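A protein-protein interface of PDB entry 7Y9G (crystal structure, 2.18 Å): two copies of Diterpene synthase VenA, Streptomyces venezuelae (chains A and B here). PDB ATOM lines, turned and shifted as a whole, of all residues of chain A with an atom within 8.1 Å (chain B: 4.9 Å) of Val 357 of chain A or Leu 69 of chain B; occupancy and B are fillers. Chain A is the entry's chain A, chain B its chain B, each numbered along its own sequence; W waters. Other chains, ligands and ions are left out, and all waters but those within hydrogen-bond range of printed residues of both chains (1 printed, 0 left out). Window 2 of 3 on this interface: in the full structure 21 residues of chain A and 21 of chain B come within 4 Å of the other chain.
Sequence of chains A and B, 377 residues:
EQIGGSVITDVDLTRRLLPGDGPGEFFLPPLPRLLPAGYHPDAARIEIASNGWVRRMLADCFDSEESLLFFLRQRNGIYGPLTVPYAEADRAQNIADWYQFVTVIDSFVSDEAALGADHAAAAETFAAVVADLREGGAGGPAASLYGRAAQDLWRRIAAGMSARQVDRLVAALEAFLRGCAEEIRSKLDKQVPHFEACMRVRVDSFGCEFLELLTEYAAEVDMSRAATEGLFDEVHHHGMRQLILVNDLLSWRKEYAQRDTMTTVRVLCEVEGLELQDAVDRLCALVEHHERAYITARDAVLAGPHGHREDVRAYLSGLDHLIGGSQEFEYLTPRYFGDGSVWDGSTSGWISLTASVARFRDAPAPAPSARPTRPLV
The backbone carbonyl oxygen (O) of Gly 340 of chain A sits at hydrogen-bond distance from the guanidinium group (NH1) of Arg 73 of chain B, at 2.8 Å. The side-chain carboxylate of Asp 344 of chain A is in salt-bridge range of the guanidinium group of Arg 55 of chain B. The side-chain carboxylate of Glu 65 of chain B lies within salt-bridge range of the guanidinium group of Arg 359 of chain A (3.2 Å). The guanidinium group (NE) of Arg 359 of chain A lies close to the guanidinium group (NH1) of Arg 55 of chain B (3.4 Å).
The guanidinium group of Arg 55 of chain B is in salt-bridge range of the side-chain carboxylate of Glu 65 of chain B (2.7 Å).
O of Gly 340 of chain A touches CB of Leu 69 of chain B, at 3.9 Å. Val 342 of chain A touches Leu 69 of chain B (N to CD2, 3.9 Å). CG1 of Val 342 of chain A touches CB of Leu 72 of chain B (3.7 Å). Arg 73 of chain B touches Val 342 of chain A (CG to CG2, 3.3 Å). Leu 69 of chain B touches Val 357 of chain A (CD1 to CG2, 3.99 Å).
Printed residues of chain B within 4 Å of Val 342 of chain A: Leu 69, Leu 72 and Arg 73. Of the printed residues of chain B, Asp 344 of chain A touches Arg 55 (2.9 Å). Of the printed residues of chain A, Glu 65 of chain B touches Arg 359 (3.2 Å). Of the printed residues of chain A, Leu 69 of chain B touches Gly 340, Val 342 and Val 357. Printed residues of chain A within 4 Å of Arg 73 of chain B: Gly 340 and Val 342. The nearest printed residue of chain A that does not touch Glu 65 of chain B is Arg 361 of chain A (4.3 Å).
Printed residues of chain B that touch a printed residue of chain A: Arg 55, Glu 65, Leu 69, Leu 72 and Arg 73. Hydrophobic or aromatic side chains of chain B within 4 Å of the printed part of chain A: Leu 69 and Leu 72. Hydrophobic or aromatic side chains of chain A within 4 Å of the printed part of chain B: Val 342 and Val 357.
No position is printed for both chains.
Water W1 lies within hydrogen-bond range of O of Val 342 of chain A, OD2 of Asp 344 of chain A and NH2 of Arg 55 of chain B.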
ATOM      1  N   ARG A 253     -13.189 -20.099  -1.747  1.00  0.00           N
ATOM      2  CA  ARG A 253     -11.987 -19.222  -1.737  1.00  0.00           C
ATOM      3  C   ARG A 253     -10.798 -20.043  -1.242  1.00  0.00           C
ATOM      4  O   ARG A 253      -9.731 -20.024  -1.890  1.00  0.00           O
ATOM      5  CB  ARG A 253     -12.215 -18.028  -0.810  1.00  0.00           C
ATOM      6  CG  ARG A 253     -11.807 -16.689  -1.382  1.00  0.00           C
ATOM      7  CD  ARG A 253     -11.961 -15.595  -0.349  1.00  0.00           C
ATOM      8  NE  ARG A 253     -10.741 -15.478   0.429  1.00  0.00           N
ATOM      9  CZ  ARG A 253      -9.633 -14.872   0.028  1.00  0.00           C
ATOM     10  NH1 ARG A 253      -9.553 -14.294  -1.160  1.00  0.00           N
ATOM     11  NH2 ARG A 253      -8.591 -14.855   0.833  1.00  0.00           N
ATOM     12  N   PRO A 334     -12.540 -15.938   9.573  1.00  0.00           N
ATOM     13  CA  PRO A 334     -11.345 -15.791   8.748  1.00  0.00           C
ATOM     14  C   PRO A 334     -10.817 -17.068   8.091  1.00  0.00           C
ATOM     15  O   PRO A 334      -9.951 -16.965   7.239  1.00  0.00           O
ATOM     16  CB  PRO A 334     -10.348 -15.258   9.766  1.00  0.00           C
ATOM     17  CG  PRO A 334     -11.227 -14.403  10.651  1.00  0.00           C
ATOM     18  CD  PRO A 334     -12.386 -15.329  10.903  1.00  0.00           C
ATOM     19  N   TYR A 336     -12.337 -18.631   5.955  1.00  0.00           N
ATOM     20  CA  TYR A 336     -12.818 -18.534   4.548  1.00  0.00           C
ATOM     21  C   TYR A 336     -12.417 -17.185   3.944  1.00  0.00           C
ATOM     22  O   TYR A 336     -12.062 -17.129   2.740  1.00  0.00           O
ATOM     23  CB  TYR A 336     -14.328 -18.787   4.493  1.00  0.00           C
ATOM     24  CG  TYR A 336     -14.744 -20.101   5.104  1.00  0.00           C
ATOM     25  CD1 TYR A 336     -13.919 -21.220   5.084  1.00  0.00           C
ATOM     26  CD2 TYR A 336     -15.969 -20.231   5.712  1.00  0.00           C
ATOM     27  CE1 TYR A 336     -14.314 -22.429   5.648  1.00  0.00           C
ATOM     28  CE2 TYR A 336     -16.374 -21.423   6.283  1.00  0.00           C
ATOM     29  CZ  TYR A 336     -15.546 -22.529   6.261  1.00  0.00           C
ATOM     30  OH  TYR A 336     -15.974 -23.679   6.858  1.00  0.00           O
ATOM     31  N   PHE A 337     -12.418 -16.112   4.739  1.00  0.00           N
ATOM     32  CA  PHE A 337     -12.252 -14.753   4.179  1.00  0.00           C
ATOM     33  C   PHE A 337     -10.795 -14.293   4.310  1.00  0.00           C
ATOM     34  O   PHE A 337     -10.505 -13.147   3.967  1.00  0.00           O
ATOM     35  CB  PHE A 337     -13.294 -13.829   4.819  1.00  0.00           C
ATOM     36  CG  PHE A 337     -14.672 -14.137   4.333  1.00  0.00           C
ATOM     37  CD1 PHE A 337     -15.122 -13.609   3.134  1.00  0.00           C
ATOM     38  CD2 PHE A 337     -15.469 -15.048   5.016  1.00  0.00           C
ATOM     39  CE1 PHE A 337     -16.372 -13.957   2.643  1.00  0.00           C
ATOM     40  CE2 PHE A 337     -16.710 -15.401   4.516  1.00  0.00           C
ATOM     41  CZ  PHE A 337     -17.166 -14.839   3.346  1.00  0.00           C
ATOM     42  N   GLY A 338      -9.925 -15.147   4.837  1.00  0.00           N
ATOM     43  CA  GLY A 338      -8.471 -14.911   4.913  1.00  0.00           C
ATOM     44  C   GLY A 338      -8.057 -14.448   6.298  1.00  0.00           C
ATOM     45  O   GLY A 338      -8.821 -13.771   6.985  1.00  0.00           O
ATOM     46  N   ASP A 339      -6.873 -14.841   6.705  1.00  0.00           N
ATOM     47  CA  ASP A 339      -6.295 -14.473   8.004  1.00  0.00           C
ATOM     48  C   ASP A 339      -6.205 -12.953   8.008  1.00  0.00           C
ATOM     49  O   ASP A 339      -5.814 -12.393   6.952  1.00  0.00           O
ATOM     50  CB  ASP A 339      -4.948 -15.153   8.191  1.00  0.00           C
ATOM     51  CG  ASP A 339      -4.414 -14.914   9.580  1.00  0.00           C
ATOM     52  OD1 ASP A 339      -5.245 -14.976  10.537  1.00  0.00           O
ATOM     53  OD2 ASP A 339      -3.195 -14.620   9.688  1.00  0.00           O
ATOM     54  N   GLY A 340      -6.651 -12.326   9.092  1.00  0.00           N
ATOM     55  CA  GLY A 340      -6.668 -10.859   9.202  1.00  0.00           C
ATOM     56  C   GLY A 340      -8.018 -10.287   8.861  1.00  0.00           C
ATOM     57  O   GLY A 340      -8.226  -9.131   9.190  1.00  0.00           O
ATOM     58  N   SER A 341      -8.902 -11.049   8.197  1.00  0.00           N
ATOM     59  CA  SER A 341     -10.283 -10.588   7.870  1.00  0.00           C
ATOM     60  C   SER A 341     -11.075 -10.369   9.161  1.00  0.00           C
ATOM     61  O   SER A 341     -10.779 -11.024  10.187  1.00  0.00           O
ATOM     62  CB  SER A 341     -11.022 -11.512   6.935  1.00  0.00           C
ATOM     63  OG  SER A 341     -11.157 -12.813   7.478  1.00  0.00           O
ATOM     64  N   VAL A 342     -12.071  -9.486   9.083  1.00  0.00           N
ATOM     65  CA  VAL A 342     -13.008  -9.144  10.189  1.00  0.00           C
ATOM     66  C   VAL A 342     -14.381  -8.934   9.561  1.00  0.00           C
ATOM     67  O   VAL A 342     -14.537  -8.034   8.716  1.00  0.00           O
ATOM     68  CB  VAL A 342     -12.576  -7.908  11.008  1.00  0.00           C
ATOM     69  CG1 VAL A 342     -13.513  -7.689  12.183  1.00  0.00           C
ATOM     70  CG2 VAL A 342     -11.147  -8.008  11.499  1.00  0.00           C
ATOM     71  N   TRP A 343     -15.360  -9.735   9.978  1.00  0.00           N
ATOM     72  CA  TRP A 343     -16.709  -9.690   9.362  1.00  0.00           C
ATOM     73  C   TRP A 343     -17.361  -8.349   9.675  1.00  0.00           C
ATOM     74  O   TRP A 343     -17.305  -7.940  10.842  1.00  0.00           O
ATOM     75  CB  TRP A 343     -17.559 -10.852   9.825  1.00  0.00           C
ATOM     76  CG  TRP A 343     -18.796 -11.011   9.000  1.00  0.00           C
ATOM     77  CD1 TRP A 343     -18.950 -10.716   7.676  1.00  0.00           C
ATOM     78  CD2 TRP A 343     -20.067 -11.493   9.461  1.00  0.00           C
ATOM     79  NE1 TRP A 343     -20.234 -10.976   7.290  1.00  0.00           N
ATOM     80  CE2 TRP A 343     -20.945 -11.451   8.357  1.00  0.00           C
ATOM     81  CE3 TRP A 343     -20.549 -11.946  10.691  1.00  0.00           C
ATOM     82  CZ2 TRP A 343     -22.276 -11.849   8.453  1.00  0.00           C
ATOM     83  CZ3 TRP A 343     -21.865 -12.349  10.784  1.00  0.00           C
ATOM     84  CH2 TRP A 343     -22.717 -12.306   9.675  1.00  0.00           C
ATOM     85  N   ASP A 344     -17.932  -7.700   8.661  1.00  0.00           N
ATOM     86  CA  ASP A 344     -18.628  -6.394   8.800  1.00  0.00           C
ATOM     87  C   ASP A 344     -20.145  -6.581   8.712  1.00  0.00           C
ATOM     88  O   ASP A 344     -20.826  -5.562   8.667  1.00  0.00           O
ATOM     89  CB  ASP A 344     -18.125  -5.396   7.760  1.00  0.00           C
ATOM     90  CG  ASP A 344     -18.335  -5.846   6.336  1.00  0.00           C
ATOM     91  OD1 ASP A 344     -19.182  -6.743   6.114  1.00  0.00           O
ATOM     92  OD2 ASP A 344     -17.596  -5.334   5.474  1.00  0.00           O
ATOM     93  N   ILE A 351     -16.698 -11.346  -4.481  1.00  0.00           N
ATOM     94  CA  ILE A 351     -15.638 -11.975  -3.641  1.00  0.00           C
ATOM     95  C   ILE A 351     -14.388 -12.205  -4.488  1.00  0.00           C
ATOM     96  O   ILE A 351     -14.496 -12.936  -5.491  1.00  0.00           O
ATOM     97  CB  ILE A 351     -16.158 -13.298  -3.047  1.00  0.00           C
ATOM     98  CG1 ILE A 351     -17.183 -13.039  -1.953  1.00  0.00           C
ATOM     99  CG2 ILE A 351     -15.010 -14.159  -2.539  1.00  0.00           C
ATOM    100  CD1 ILE A 351     -16.580 -12.395  -0.709  1.00  0.00           C
ATOM    101  N   SER A 352     -13.248 -11.665  -4.057  1.00  0.00           N
ATOM    102  CA  SER A 352     -11.925 -11.925  -4.673  1.00  0.00           C
ATOM    103  C   SER A 352     -11.434 -13.321  -4.282  1.00  0.00           C
ATOM    104  O   SER A 352     -11.454 -13.674  -3.073  1.00  0.00           O
ATOM    105  CB  SER A 352     -10.900 -10.882  -4.305  1.00  0.00           C
ATOM    106  OG  SER A 352      -9.629 -11.200  -4.860  1.00  0.00           O
ATOM    107  N   LEU A 353     -10.964 -14.064  -5.280  1.00  0.00           N
ATOM    108  CA  LEU A 353     -10.291 -15.366  -5.098  1.00  0.00           C
ATOM    109  C   LEU A 353      -8.799 -15.172  -4.840  1.00  0.00           C
ATOM    110  O   LEU A 353      -8.177 -16.115  -4.340  1.00  0.00           O
ATOM    111  CB  LEU A 353     -10.503 -16.188  -6.364  1.00  0.00           C
ATOM    112  CG  LEU A 353     -11.872 -16.827  -6.500  1.00  0.00           C
ATOM    113  CD1 LEU A 353     -11.924 -17.630  -7.787  1.00  0.00           C
ATOM    114  CD2 LEU A 353     -12.171 -17.710  -5.295  1.00  0.00           C
ATOM    115  N   THR A 354      -8.237 -14.014  -5.189  1.00  0.00           N
ATOM    116  CA  THR A 354      -6.764 -13.802  -5.204  1.00  0.00           C
ATOM    117  C   THR A 354      -6.341 -12.968  -3.997  1.00  0.00           C
ATOM    118  O   THR A 354      -5.249 -13.198  -3.484  1.00  0.00           O
ATOM    119  CB  THR A 354      -6.317 -13.226  -6.550  1.00  0.00           C
ATOM    120  OG1 THR A 354      -7.071 -12.062  -6.899  1.00  0.00           O
ATOM    121  CG2 THR A 354      -6.486 -14.246  -7.653  1.00  0.00           C
ATOM    122  N   ALA A 355      -7.181 -12.051  -3.531  1.00  0.00           N
ATOM    123  CA  ALA A 355      -6.844 -11.172  -2.394  1.00  0.00           C
ATOM    124  C   ALA A 355      -6.430 -12.027  -1.198  1.00  0.00           C
ATOM    125  O   ALA A 355      -6.971 -13.127  -1.022  1.00  0.00           O
ATOM    126  CB  ALA A 355      -8.018 -10.284  -2.074  1.00  0.00           C
ATOM    127  N   SER A 356      -5.523 -11.504  -0.387  1.00  0.00           N
ATOM    128  CA  SER A 356      -5.045 -12.096   0.880  1.00  0.00           C
ATOM    129  C   SER A 356      -6.163 -12.057   1.941  1.00  0.00           C
ATOM    130  O   SER A 356      -6.173 -12.923   2.838  1.00  0.00           O
ATOM    131  CB  SER A 356      -3.799 -11.373   1.328  1.00  0.00           C
ATOM    132  OG  SER A 356      -4.093 -10.070   1.831  1.00  0.00           O
ATOM    133  N   VAL A 357      -7.042 -11.063   1.860  1.00  0.00           N
ATOM    134  CA  VAL A 357      -8.257 -10.918   2.705  1.00  0.00           C
ATOM    135  C   VAL A 357      -9.416 -10.555   1.775  1.00  0.00           C
ATOM    136  O   VAL A 357      -9.220  -9.767   0.853  1.00  0.00           O
ATOM    137  CB  VAL A 357      -8.088  -9.862   3.812  1.00  0.00           C
ATOM    138  CG1 VAL A 357      -7.306 -10.394   4.985  1.00  0.00           C
ATOM    139  CG2 VAL A 357      -7.455  -8.588   3.305  1.00  0.00           C
ATOM    140  N   ALA A 358     -10.582 -11.143   1.981  1.00  0.00           N
ATOM    141  CA  ALA A 358     -11.760 -10.890   1.125  1.00  0.00           C
ATOM    142  C   ALA A 358     -12.929 -10.479   2.002  1.00  0.00           C
ATOM    143  O   ALA A 358     -12.963 -10.809   3.212  1.00  0.00           O
ATOM    144  CB  ALA A 358     -12.098 -12.115   0.301  1.00  0.00           C
ATOM    145  N   ARG A 359     -13.865  -9.784   1.377  1.00  0.00           N
ATOM    146  CA  ARG A 359     -15.154  -9.373   1.964  1.00  0.00           C
ATOM    147  C   ARG A 359     -16.071  -9.126   0.783  1.00  0.00           C
ATOM    148  O   ARG A 359     -15.521  -8.948  -0.324  1.00  0.00           O
ATOM    149  CB  ARG A 359     -14.975  -8.111   2.809  1.00  0.00           C
ATOM    150  CG  ARG A 359     -14.842  -6.829   2.002  1.00  0.00           C
ATOM    151  CD  ARG A 359     -14.355  -5.682   2.870  1.00  0.00           C
ATOM    152  NE  ARG A 359     -13.910  -4.546   2.078  1.00  0.00           N
ATOM    153  CZ  ARG A 359     -14.725  -3.676   1.489  1.00  0.00           C
ATOM    154  NH1 ARG A 359     -16.034  -3.797   1.619  1.00  0.00           N
ATOM    155  NH2 ARG A 359     -14.226  -2.680   0.781  1.00  0.00           N
ATOM    156  N   ARG A 361     -18.251  -7.046  -1.709  1.00  0.00           N
ATOM    157  CA  ARG A 361     -18.250  -5.655  -2.257  1.00  0.00           C
ATOM    158  C   ARG A 361     -19.414  -5.479  -3.253  1.00  0.00           C
ATOM    159  O   ARG A 361     -19.828  -6.482  -3.852  1.00  0.00           O
ATOM    160  CB  ARG A 361     -16.906  -5.363  -2.938  1.00  0.00           C
ATOM    161  CG  ARG A 361     -15.724  -5.201  -1.986  1.00  0.00           C
ATOM    162  CD  ARG A 361     -14.480  -4.679  -2.698  1.00  0.00           C
ATOM    163  NE  ARG A 361     -13.448  -4.099  -1.835  1.00  0.00           N
ATOM    164  CZ  ARG A 361     -12.562  -4.787  -1.101  1.00  0.00           C
ATOM    165  NH1 ARG A 361     -11.661  -4.163  -0.358  1.00  0.00           N
ATOM    166  NH2 ARG A 361     -12.583  -6.098  -1.090  1.00  0.00           N
ATOM    167  N   ARG B  55     -17.224   0.560   9.099  1.00  0.00           N
ATOM    168  CA  ARG B  55     -16.889   0.530   7.654  1.00  0.00           C
ATOM    169  C   ARG B  55     -17.698   1.631   6.940  1.00  0.00           C
ATOM    170  O   ARG B  55     -17.065   2.514   6.367  1.00  0.00           O
ATOM    171  CB  ARG B  55     -17.104  -0.842   7.016  1.00  0.00           C
ATOM    172  CG  ARG B  55     -16.936  -0.797   5.501  1.00  0.00           C
ATOM    173  CD  ARG B  55     -16.940  -2.131   4.786  1.00  0.00           C
ATOM    174  NE  ARG B  55     -15.902  -3.008   5.268  1.00  0.00           N
ATOM    175  CZ  ARG B  55     -14.605  -2.916   4.981  1.00  0.00           C
ATOM    176  NH1 ARG B  55     -14.134  -1.929   4.234  1.00  0.00           N
ATOM    177  NH2 ARG B  55     -13.768  -3.804   5.494  1.00  0.00           N
ATOM    178  N   GLU B  65      -7.532  -0.580   3.566  1.00  0.00           N
ATOM    179  CA  GLU B  65      -8.274  -1.735   4.106  1.00  0.00           C
ATOM    180  C   GLU B  65      -7.415  -2.393   5.184  1.00  0.00           C
ATOM    181  O   GLU B  65      -7.978  -2.792   6.206  1.00  0.00           O
ATOM    182  CB  GLU B  65      -8.627  -2.657   2.945  1.00  0.00           C
ATOM    183  CG  GLU B  65      -9.442  -3.843   3.368  1.00  0.00           C
ATOM    184  CD  GLU B  65     -10.863  -3.511   3.790  1.00  0.00           C
ATOM    185  OE1 GLU B  65     -11.291  -2.336   3.675  1.00  0.00           O
ATOM    186  OE2 GLU B  65     -11.534  -4.443   4.215  1.00  0.00           O
ATOM    187  N   GLU B  66      -6.096  -2.431   4.988  1.00  0.00           N
ATOM    188  CA  GLU B  66      -5.111  -3.024   5.936  1.00  0.00           C
ATOM    189  C   GLU B  66      -5.226  -2.297   7.287  1.00  0.00           C
ATOM    190  O   GLU B  66      -5.190  -2.963   8.350  1.00  0.00           O
ATOM    191  CB  GLU B  66      -3.718  -2.948   5.298  1.00  0.00           C
ATOM    192  CG  GLU B  66      -2.548  -3.145   6.247  1.00  0.00           C
ATOM    193  CD  GLU B  66      -1.253  -2.481   5.781  1.00  0.00           C
ATOM    194  OE1 GLU B  66      -0.715  -2.879   4.704  1.00  0.00           O
ATOM    195  OE2 GLU B  66      -0.787  -1.549   6.491  1.00  0.00           O
ATOM    196  N   SER B  67      -5.363  -0.975   7.241  1.00  0.00           N
ATOM    197  CA  SER B  67      -5.416  -0.082   8.430  1.00  0.00           C
ATOM    198  C   SER B  67      -6.756  -0.248   9.152  1.00  0.00           C
ATOM    199  O   SER B  67      -6.755  -0.397  10.373  1.00  0.00           O
ATOM    200  CB  SER B  67      -5.171   1.356   8.019  1.00  0.00           C
ATOM    201  OG  SER B  67      -3.787   1.603   8.051  1.00  0.00           O
ATOM    202  N   LEU B  68      -7.849  -0.244   8.393  1.00  0.00           N
ATOM    203  CA  LEU B  68      -9.225  -0.496   8.892  1.00  0.00           C
ATOM    204  C   LEU B  68      -9.265  -1.847   9.629  1.00  0.00           C
ATOM    205  O   LEU B  68      -9.647  -1.875  10.822  1.00  0.00           O
ATOM    206  CB  LEU B  68     -10.178  -0.466   7.699  1.00  0.00           C
ATOM    207  CG  LEU B  68     -11.619  -0.845   8.016  1.00  0.00           C
ATOM    208  CD1 LEU B  68     -12.200   0.115   9.052  1.00  0.00           C
ATOM    209  CD2 LEU B  68     -12.453  -0.840   6.747  1.00  0.00           C
ATOM    210  N   LEU B  69      -8.810  -2.921   8.988  1.00  0.00           N
ATOM    211  CA  LEU B  69      -8.864  -4.290   9.573  1.00  0.00           C
ATOM    212  C   LEU B  69      -7.985  -4.389  10.830  1.00  0.00           C
ATOM    213  O   LEU B  69      -8.438  -5.022  11.816  1.00  0.00           O
ATOM    214  CB  LEU B  69      -8.467  -5.318   8.514  1.00  0.00           C
ATOM    215  CG  LEU B  69      -9.449  -5.427   7.352  1.00  0.00           C
ATOM    216  CD1 LEU B  69      -8.871  -6.285   6.236  1.00  0.00           C
ATOM    217  CD2 LEU B  69     -10.785  -5.997   7.806  1.00  0.00           C
ATOM    218  N   PHE B  70      -6.815  -3.750  10.851  1.00  0.00           N
ATOM    219  CA  PHE B  70      -5.984  -3.613  12.076  1.00  0.00           C
ATOM    220  C   PHE B  70      -6.874  -3.115  13.226  1.00  0.00           C
ATOM    221  O   PHE B  70      -6.870  -3.699  14.354  1.00  0.00           O
ATOM    222  CB  PHE B  70      -4.788  -2.674  11.871  1.00  0.00           C
ATOM    223  CG  PHE B  70      -3.912  -2.501  13.088  1.00  0.00           C
ATOM    224  CD1 PHE B  70      -2.895  -3.396  13.362  1.00  0.00           C
ATOM    225  CD2 PHE B  70      -4.100  -1.443  13.961  1.00  0.00           C
ATOM    226  CE1 PHE B  70      -2.080  -3.246  14.476  1.00  0.00           C
ATOM    227  CE2 PHE B  70      -3.295  -1.290  15.078  1.00  0.00           C
ATOM    228  CZ  PHE B  70      -2.281  -2.188  15.327  1.00  0.00           C
ATOM    229  N   PHE B  71      -7.663  -2.079  12.948  1.00  0.00           N
ATOM    230  CA  PHE B  71      -8.570  -1.480  13.951  1.00  0.00           C
ATOM    231  C   PHE B  71      -9.692  -2.466  14.313  1.00  0.00           C
ATOM    232  O   PHE B  71      -9.973  -2.675  15.503  1.00  0.00           O
ATOM    233  CB  PHE B  71      -9.141  -0.153  13.457  1.00  0.00           C
ATOM    234  CG  PHE B  71      -9.966   0.505  14.524  1.00  0.00           C
ATOM    235  CD1 PHE B  71      -9.346   1.155  15.575  1.00  0.00           C
ATOM    236  CD2 PHE B  71     -11.345   0.376  14.533  1.00  0.00           C
ATOM    237  CE1 PHE B  71     -10.102   1.730  16.585  1.00  0.00           C
ATOM    238  CE2 PHE B  71     -12.102   0.936  15.558  1.00  0.00           C
ATOM    239  CZ  PHE B  71     -11.479   1.621  16.579  1.00  0.00           C
ATOM    240  N   LEU B  72     -10.309  -3.083  13.311  1.00  0.00           N
ATOM    241  CA  LEU B  72     -11.439  -4.010  13.532  1.00  0.00           C
ATOM    242  C   LEU B  72     -10.960  -5.257  14.280  1.00  0.00           C
ATOM    243  O   LEU B  72     -11.773  -5.825  15.049  1.00  0.00           O
ATOM    244  CB  LEU B  72     -12.112  -4.309  12.187  1.00  0.00           C
ATOM    245  CG  LEU B  72     -12.790  -3.102  11.538  1.00  0.00           C
ATOM    246  CD1 LEU B  72     -13.558  -3.530  10.313  1.00  0.00           C
ATOM    247  CD2 LEU B  72     -13.708  -2.384  12.508  1.00  0.00           C
ATOM    248  N   ARG B  73      -9.689  -5.637  14.143  1.00  0.00           N
ATOM    249  CA  ARG B  73      -9.168  -6.868  14.787  1.00  0.00           C
ATOM    250  C   ARG B  73      -8.980  -6.610  16.277  1.00  0.00           C
ATOM    251  O   ARG B  73      -8.877  -7.598  17.016  1.00  0.00           O
ATOM    252  CB  ARG B  73      -7.872  -7.365  14.150  1.00  0.00           C
ATOM    253  CG  ARG B  73      -8.083  -8.078  12.819  1.00  0.00           C
ATOM    254  CD  ARG B  73      -6.851  -8.850  12.410  1.00  0.00           C
ATOM    255  NE  ARG B  73      -5.698  -7.978  12.216  1.00  0.00           N
ATOM    256  CZ  ARG B  73      -5.355  -7.376  11.078  1.00  0.00           C
ATOM    257  NH1 ARG B  73      -6.077  -7.524   9.981  1.00  0.00           N
ATOM    258  NH2 ARG B  73      -4.264  -6.629  11.038  1.00  0.00           N
HETATM  259  O   HOH W   1     -14.989  -6.488   6.737  1.00  0.00           O
